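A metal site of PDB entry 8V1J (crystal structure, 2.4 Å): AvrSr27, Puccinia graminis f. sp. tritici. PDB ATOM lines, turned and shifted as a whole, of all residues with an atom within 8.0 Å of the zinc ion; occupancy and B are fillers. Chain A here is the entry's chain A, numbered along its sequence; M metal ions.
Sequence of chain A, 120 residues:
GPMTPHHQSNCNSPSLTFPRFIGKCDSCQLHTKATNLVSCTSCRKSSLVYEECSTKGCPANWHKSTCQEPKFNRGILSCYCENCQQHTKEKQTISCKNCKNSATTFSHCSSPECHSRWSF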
ATOM      1  N   CYS A  79       4.788   5.431 -28.588  1.00  0.00           N
ATOM      2  CA  CYS A  79       4.631   6.339 -27.461  1.00  0.00           C
ATOM      3  C   CYS A  79       5.807   6.216 -26.508  1.00  0.00           C
ATOM      4  O   CYS A  79       6.561   5.241 -26.528  1.00  0.00           O
ATOM      5  CB  CYS A  79       3.352   6.057 -26.687  1.00  0.00           C
ATOM      6  SG  CYS A  79       2.036   5.379 -27.696  1.00  0.00           S
ATOM      7  N   TYR A  80       5.943   7.230 -25.647  1.00  0.00           N
ATOM      8  CA  TYR A  80       6.800   7.124 -24.484  1.00  0.00           C
ATOM      9  C   TYR A  80       6.033   6.444 -23.353  1.00  0.00           C
ATOM     10  O   TYR A  80       4.855   6.739 -23.113  1.00  0.00           O
ATOM     11  CB  TYR A  80       7.289   8.503 -24.037  1.00  0.00           C
ATOM     12  CG  TYR A  80       8.445   9.023 -24.855  1.00  0.00           C
ATOM     13  CD1 TYR A  80       8.287  10.113 -25.709  1.00  0.00           C
ATOM     14  CD2 TYR A  80       9.698   8.423 -24.787  1.00  0.00           C
ATOM     15  CE1 TYR A  80       9.349  10.586 -26.456  1.00  0.00           C
ATOM     16  CE2 TYR A  80      10.759   8.896 -25.535  1.00  0.00           C
ATOM     17  CZ  TYR A  80      10.580   9.974 -26.371  1.00  0.00           C
ATOM     18  OH  TYR A  80      11.628  10.450 -27.116  1.00  0.00           O
ATOM     19  N   CYS A  81       6.704   5.537 -22.656  1.00  0.00           N
ATOM     20  CA  CYS A  81       6.071   4.780 -21.586  1.00  0.00           C
ATOM     21  C   CYS A  81       6.101   5.556 -20.279  1.00  0.00           C
ATOM     22  O   CYS A  81       7.085   6.223 -19.955  1.00  0.00           O
ATOM     23  CB  CYS A  81       6.777   3.427 -21.400  1.00  0.00           C
ATOM     24  SG  CYS A  81       6.061   2.430 -20.081  1.00  0.00           S
ATOM     25  N   GLU A  82       5.008   5.455 -19.519  1.00  0.00           N
ATOM     26  CA  GLU A  82       4.898   6.169 -18.261  1.00  0.00           C
ATOM     27  C   GLU A  82       5.577   5.450 -17.106  1.00  0.00           C
ATOM     28  O   GLU A  82       5.743   6.046 -16.044  1.00  0.00           O
ATOM     29  CB  GLU A  82       3.422   6.392 -17.907  1.00  0.00           C
ATOM     30  CG  GLU A  82       2.500   6.595 -19.104  1.00  0.00           C
ATOM     31  CD  GLU A  82       1.817   5.304 -19.550  1.00  0.00           C
ATOM     32  OE1 GLU A  82       2.525   4.296 -19.745  1.00  0.00           O
ATOM     33  OE2 GLU A  82       0.581   5.300 -19.700  1.00  0.00           O
ATOM     34  N   ASN A  83       5.986   4.194 -17.297  1.00  0.00           N
ATOM     35  CA  ASN A  83       6.645   3.409 -16.257  1.00  0.00           C
ATOM     36  C   ASN A  83       8.161   3.407 -16.377  1.00  0.00           C
ATOM     37  O   ASN A  83       8.852   3.539 -15.371  1.00  0.00           O
ATOM     38  CB  ASN A  83       6.142   1.961 -16.284  1.00  0.00           C
ATOM     39  CG  ASN A  83       4.698   1.838 -15.849  1.00  0.00           C
ATOM     40  OD1 ASN A  83       4.366   2.038 -14.679  1.00  0.00           O
ATOM     41  ND2 ASN A  83       3.824   1.497 -16.788  1.00  0.00           N
ATOM     42  N   CYS A  84       8.691   3.244 -17.595  1.00  0.00           N
ATOM     43  CA  CYS A  84      10.135   3.155 -17.805  1.00  0.00           C
ATOM     44  C   CYS A  84      10.714   4.345 -18.541  1.00  0.00           C
ATOM     45  O   CYS A  84      11.947   4.429 -18.667  1.00  0.00           O
ATOM     46  CB  CYS A  84      10.472   1.865 -18.558  1.00  0.00           C
ATOM     47  SG  CYS A  84       9.852   1.789 -20.258  1.00  0.00           S
ATOM     48  N   GLN A  85       9.885   5.250 -19.048  1.00  0.00           N
ATOM     49  CA  GLN A  85      10.301   6.481 -19.718  1.00  0.00           C
ATOM     50  C   GLN A  85      11.077   6.223 -21.002  1.00  0.00           C
ATOM     51  O   GLN A  85      11.722   7.144 -21.524  1.00  0.00           O
ATOM     52  CB  GLN A  85      11.136   7.370 -18.782  1.00  0.00           C
ATOM     53  CG  GLN A  85      10.374   7.882 -17.577  1.00  0.00           C
ATOM     54  CD  GLN A  85      10.211   6.843 -16.483  1.00  0.00           C
ATOM     55  OE1 GLN A  85      11.129   6.085 -16.198  1.00  0.00           O
ATOM     56  NE2 GLN A  85       9.026   6.791 -15.885  1.00  0.00           N
ATOM     57  N   GLN A  86      11.028   5.010 -21.542  1.00  0.00           N
ATOM     58  CA  GLN A  86      11.632   4.709 -22.828  1.00  0.00           C
ATOM     59  C   GLN A  86      10.624   4.959 -23.949  1.00  0.00           C
ATOM     60  O   GLN A  86       9.421   5.080 -23.712  1.00  0.00           O
ATOM     61  CB  GLN A  86      12.119   3.266 -22.886  1.00  0.00           C
ATOM     62  CG  GLN A  86      13.116   2.895 -21.797  1.00  0.00           C
ATOM     63  CD  GLN A  86      14.396   3.686 -21.901  1.00  0.00           C
ATOM     64  OE1 GLN A  86      14.868   3.990 -23.006  1.00  0.00           O
ATOM     65  NE2 GLN A  86      14.973   4.026 -20.763  1.00  0.00           N
ATOM     66  N   HIS A  87      11.135   5.036 -25.170  1.00  0.00           N
ATOM     67  CA  HIS A  87      10.275   5.111 -26.350  1.00  0.00           C
ATOM     68  C   HIS A  87       9.960   3.707 -26.855  1.00  0.00           C
ATOM     69  O   HIS A  87      10.188   3.373 -28.024  1.00  0.00           O
ATOM     70  CB  HIS A  87      10.930   5.945 -27.436  1.00  0.00           C
ATOM     71  CG  HIS A  87       9.988   6.383 -28.513  1.00  0.00           C
ATOM     72  ND1 HIS A  87      10.289   6.320 -29.858  1.00  0.00           N
ATOM     73  CD2 HIS A  87       8.726   6.893 -28.436  1.00  0.00           C
ATOM     74  CE1 HIS A  87       9.269   6.766 -30.560  1.00  0.00           C
ATOM     75  NE2 HIS A  87       8.311   7.130 -29.723  1.00  0.00           N
ATOM     76  N   THR A  88       9.431   2.868 -25.962  1.00  0.00           N
ATOM     77  CA  THR A  88       9.221   1.451 -26.241  1.00  0.00           C
ATOM     78  C   THR A  88       7.761   1.035 -26.137  1.00  0.00           C
ATOM     79  O   THR A  88       7.476  -0.171 -26.157  1.00  0.00           O
ATOM     80  CB  THR A  88      10.065   0.606 -25.279  1.00  0.00           C
ATOM     81  OG1 THR A  88       9.826   1.039 -23.929  1.00  0.00           O
ATOM     82  CG2 THR A  88      11.547   0.738 -25.598  1.00  0.00           C
ATOM     83  N   LYS A  89       6.831   1.980 -26.032  1.00  0.00           N
ATOM     84  CA  LYS A  89       5.423   1.676 -25.904  1.00  0.00           C
ATOM     85  C   LYS A  89       4.741   1.707 -27.267  1.00  0.00           C
ATOM     86  O   LYS A  89       5.056   2.561 -28.105  1.00  0.00           O
ATOM     87  CB  LYS A  89       4.734   2.654 -24.960  1.00  0.00           C
ATOM     88  CG  LYS A  89       3.263   2.382 -24.730  1.00  0.00           C
ATOM     89  CD  LYS A  89       2.649   3.383 -23.766  1.00  0.00           C
ATOM     90  CE  LYS A  89       1.202   3.053 -23.456  1.00  0.00           C
ATOM     91  NZ  LYS A  89       0.642   3.931 -22.403  1.00  0.00           N
ATOM     92  N   HIS A 108       1.329  -2.093 -24.964  1.00  0.00           N
ATOM     93  CA  HIS A 108       2.427  -2.831 -24.358  1.00  0.00           C
ATOM     94  C   HIS A 108       3.696  -2.000 -24.451  1.00  0.00           C
ATOM     95  O   HIS A 108       3.815  -1.100 -25.287  1.00  0.00           O
ATOM     96  CB  HIS A 108       2.622  -4.194 -25.029  1.00  0.00           C
ATOM     97  CG  HIS A 108       3.037  -4.103 -26.466  1.00  0.00           C
ATOM     98  ND1 HIS A 108       4.343  -3.910 -26.856  1.00  0.00           N
ATOM     99  CD2 HIS A 108       2.313  -4.176 -27.609  1.00  0.00           C
ATOM    100  CE1 HIS A 108       4.406  -3.875 -28.178  1.00  0.00           C
ATOM    101  NE2 HIS A 108       3.186  -4.034 -28.655  1.00  0.00           N
ATOM    102  N   CYS A 109       4.639  -2.306 -23.575  1.00  0.00           N
ATOM    103  CA  CYS A 109       5.965  -1.708 -23.593  1.00  0.00           C
ATOM    104  C   CYS A 109       7.000  -2.826 -23.673  1.00  0.00           C
ATOM    105  O   CYS A 109       6.924  -3.798 -22.914  1.00  0.00           O
ATOM    106  CB  CYS A 109       6.194  -0.844 -22.352  1.00  0.00           C
ATOM    107  SG  CYS A 109       7.862  -0.162 -22.252  1.00  0.00           S
ATOM    108  N   SER A 110       7.961  -2.670 -24.579  1.00  0.00           N
ATOM    109  CA  SER A 110       8.937  -3.716 -24.868  1.00  0.00           C
ATOM    110  C   SER A 110      10.239  -3.552 -24.107  1.00  0.00           C
ATOM    111  O   SER A 110      11.147  -4.377 -24.281  1.00  0.00           O
ATOM    112  CB  SER A 110       9.225  -3.751 -26.367  1.00  0.00           C
ATOM    113  OG  SER A 110       9.915  -2.586 -26.781  1.00  0.00           O
ATOM    114  N   SER A 111      10.373  -2.518 -23.281  1.00  0.00           N
ATOM    115  CA  SER A 111      11.618  -2.313 -22.563  1.00  0.00           C
ATOM    116  C   SER A 111      11.895  -3.508 -21.648  1.00  0.00           C
ATOM    117  O   SER A 111      10.970  -4.209 -21.240  1.00  0.00           O
ATOM    118  CB  SER A 111      11.566  -1.028 -21.736  1.00  0.00           C
ATOM    119  OG  SER A 111      10.782  -1.200 -20.564  1.00  0.00           O
ATOM    120  N   PRO A 112      13.169  -3.767 -21.325  1.00  0.00           N
ATOM    121  CA  PRO A 112      13.443  -4.813 -20.328  1.00  0.00           C
ATOM    122  C   PRO A 112      12.624  -4.667 -19.058  1.00  0.00           C
ATOM    123  O   PRO A 112      12.073  -5.650 -18.552  1.00  0.00           O
ATOM    124  CB  PRO A 112      14.948  -4.627 -20.058  1.00  0.00           C
ATOM    125  CG  PRO A 112      15.478  -4.092 -21.336  1.00  0.00           C
ATOM    126  CD  PRO A 112      14.403  -3.197 -21.892  1.00  0.00           C
ATOM    127  N   GLU A 113      12.497  -3.434 -18.542  1.00  0.00           N
ATOM    128  CA  GLU A 113      11.812  -3.210 -17.282  1.00  0.00           C
ATOM    129  C   GLU A 113      10.338  -3.626 -17.372  1.00  0.00           C
ATOM    130  O   GLU A 113       9.831  -4.308 -16.474  1.00  0.00           O
ATOM    131  CB  GLU A 113      11.932  -1.739 -16.878  1.00  0.00           C
ATOM    132  CG  GLU A 113      11.280  -1.387 -15.549  1.00  0.00           C
ATOM    133  CD  GLU A 113      11.358   0.093 -15.229  1.00  0.00           C
ATOM    134  OE1 GLU A 113      12.316   0.747 -15.676  1.00  0.00           O
ATOM    135  OE2 GLU A 113      10.449   0.604 -14.542  1.00  0.00           O
ATOM    136  N   CYS A 114       9.654  -3.227 -18.440  1.00  0.00           N
ATOM    137  CA  CYS A 114       8.208  -3.433 -18.519  1.00  0.00           C
ATOM    138  C   CYS A 114       7.852  -4.818 -19.035  1.00  0.00           C
ATOM    139  O   CYS A 114       7.020  -5.514 -18.445  1.00  0.00           O
ATOM    140  CB  CYS A 114       7.571  -2.358 -19.399  1.00  0.00           C
ATOM    141  SG  CYS A 114       7.409  -0.747 -18.616  1.00  0.00           S
ATOM    142  N   HIS A 115       8.453  -5.232 -20.154  1.00  0.00           N
ATOM    143  CA  HIS A 115       8.042  -6.484 -20.776  1.00  0.00           C
ATOM    144  C   HIS A 115       8.333  -7.692 -19.892  1.00  0.00           C
ATOM    145  O   HIS A 115       7.681  -8.728 -20.039  1.00  0.00           O
ATOM    146  CB  HIS A 115       8.707  -6.643 -22.148  1.00  0.00           C
ATOM    147  CG  HIS A 115       9.918  -7.531 -22.156  1.00  0.00           C
ATOM    148  ND1 HIS A 115      11.191  -7.046 -21.994  1.00  0.00           N
ATOM    149  CD2 HIS A 115      10.032  -8.868 -22.328  1.00  0.00           C
ATOM    150  CE1 HIS A 115      12.049  -8.048 -22.058  1.00  0.00           C
ATOM    151  NE2 HIS A 115      11.374  -9.171 -22.262  1.00  0.00           N
ATOM    152  N   TRP A 118       5.204  -8.782 -18.077  1.00  0.00           N
ATOM    153  CA  TRP A 118       4.082  -9.321 -18.838  1.00  0.00           C
ATOM    154  C   TRP A 118       3.612 -10.630 -18.208  1.00  0.00           C
ATOM    155  O   TRP A 118       4.402 -11.405 -17.673  1.00  0.00           O
ATOM    156  CB  TRP A 118       4.486  -9.563 -20.286  1.00  0.00           C
ATOM    157  CG  TRP A 118       4.661  -8.333 -21.104  1.00  0.00           C
ATOM    158  CD1 TRP A 118       4.308  -7.054 -20.756  1.00  0.00           C
ATOM    159  CD2 TRP A 118       5.223  -8.248 -22.415  1.00  0.00           C
ATOM    160  NE1 TRP A 118       4.622  -6.184 -21.780  1.00  0.00           N
ATOM    161  CE2 TRP A 118       5.185  -6.899 -22.812  1.00  0.00           C
ATOM    162  CE3 TRP A 118       5.769  -9.195 -23.299  1.00  0.00           C
ATOM    163  CZ2 TRP A 118       5.665  -6.465 -24.040  1.00  0.00           C
ATOM    164  CZ3 TRP A 118       6.235  -8.758 -24.525  1.00  0.00           C
ATOM    165  CH2 TRP A 118       6.188  -7.408 -24.887  1.00  0.00           C
HETATM  166 ZN    ZN M   1       7.747   0.877 -20.288  1.00  0.00          ZN
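SG of Cys 84 sits close to N of Gln 86. SG of Cys 109 sits close to OG1 of Thr 88, at 2.8 Å. The backbone carbonyl oxygen of Ser 111 sits at hydrogen-bond distance from a ring nitrogen (ND1) of His 115. SG of Cys 81 sits close to N of Asn 83 (3.3 Å). The backbone carbonyl oxygen (O) of Cys 109 lies close to the backbone NH (N) of His 115 (3.5 Å). The backbone NH of Cys 81 sits at hydrogen-bond distance from the backbone carbonyl oxygen of Gln 86. The side-chain sulfur (SG) of Cys 84 sits close to the side-chain hydroxyl (OG) of Ser 111. OG of Ser 111 lies close to N of Glu 113.
SG of Cys 109 binds the zinc ion. The side-chain sulfur (SG) of Cys 84 binds the zinc ion, 2.3 Å away. SG of Cys 81 binds the zinc ion. The side-chain sulfur (SG) of Cys 114 is bound to the zinc ion, 2.4 Å away. The zinc ion has four donor atoms within binding distance.
Ser 111 touches the zinc ion. Of the 20 residues printed, 5 come within 4 Å of the zinc ion. The nearest printed residue that does not touch the zinc ion is Thr 88 (4.2 Å).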
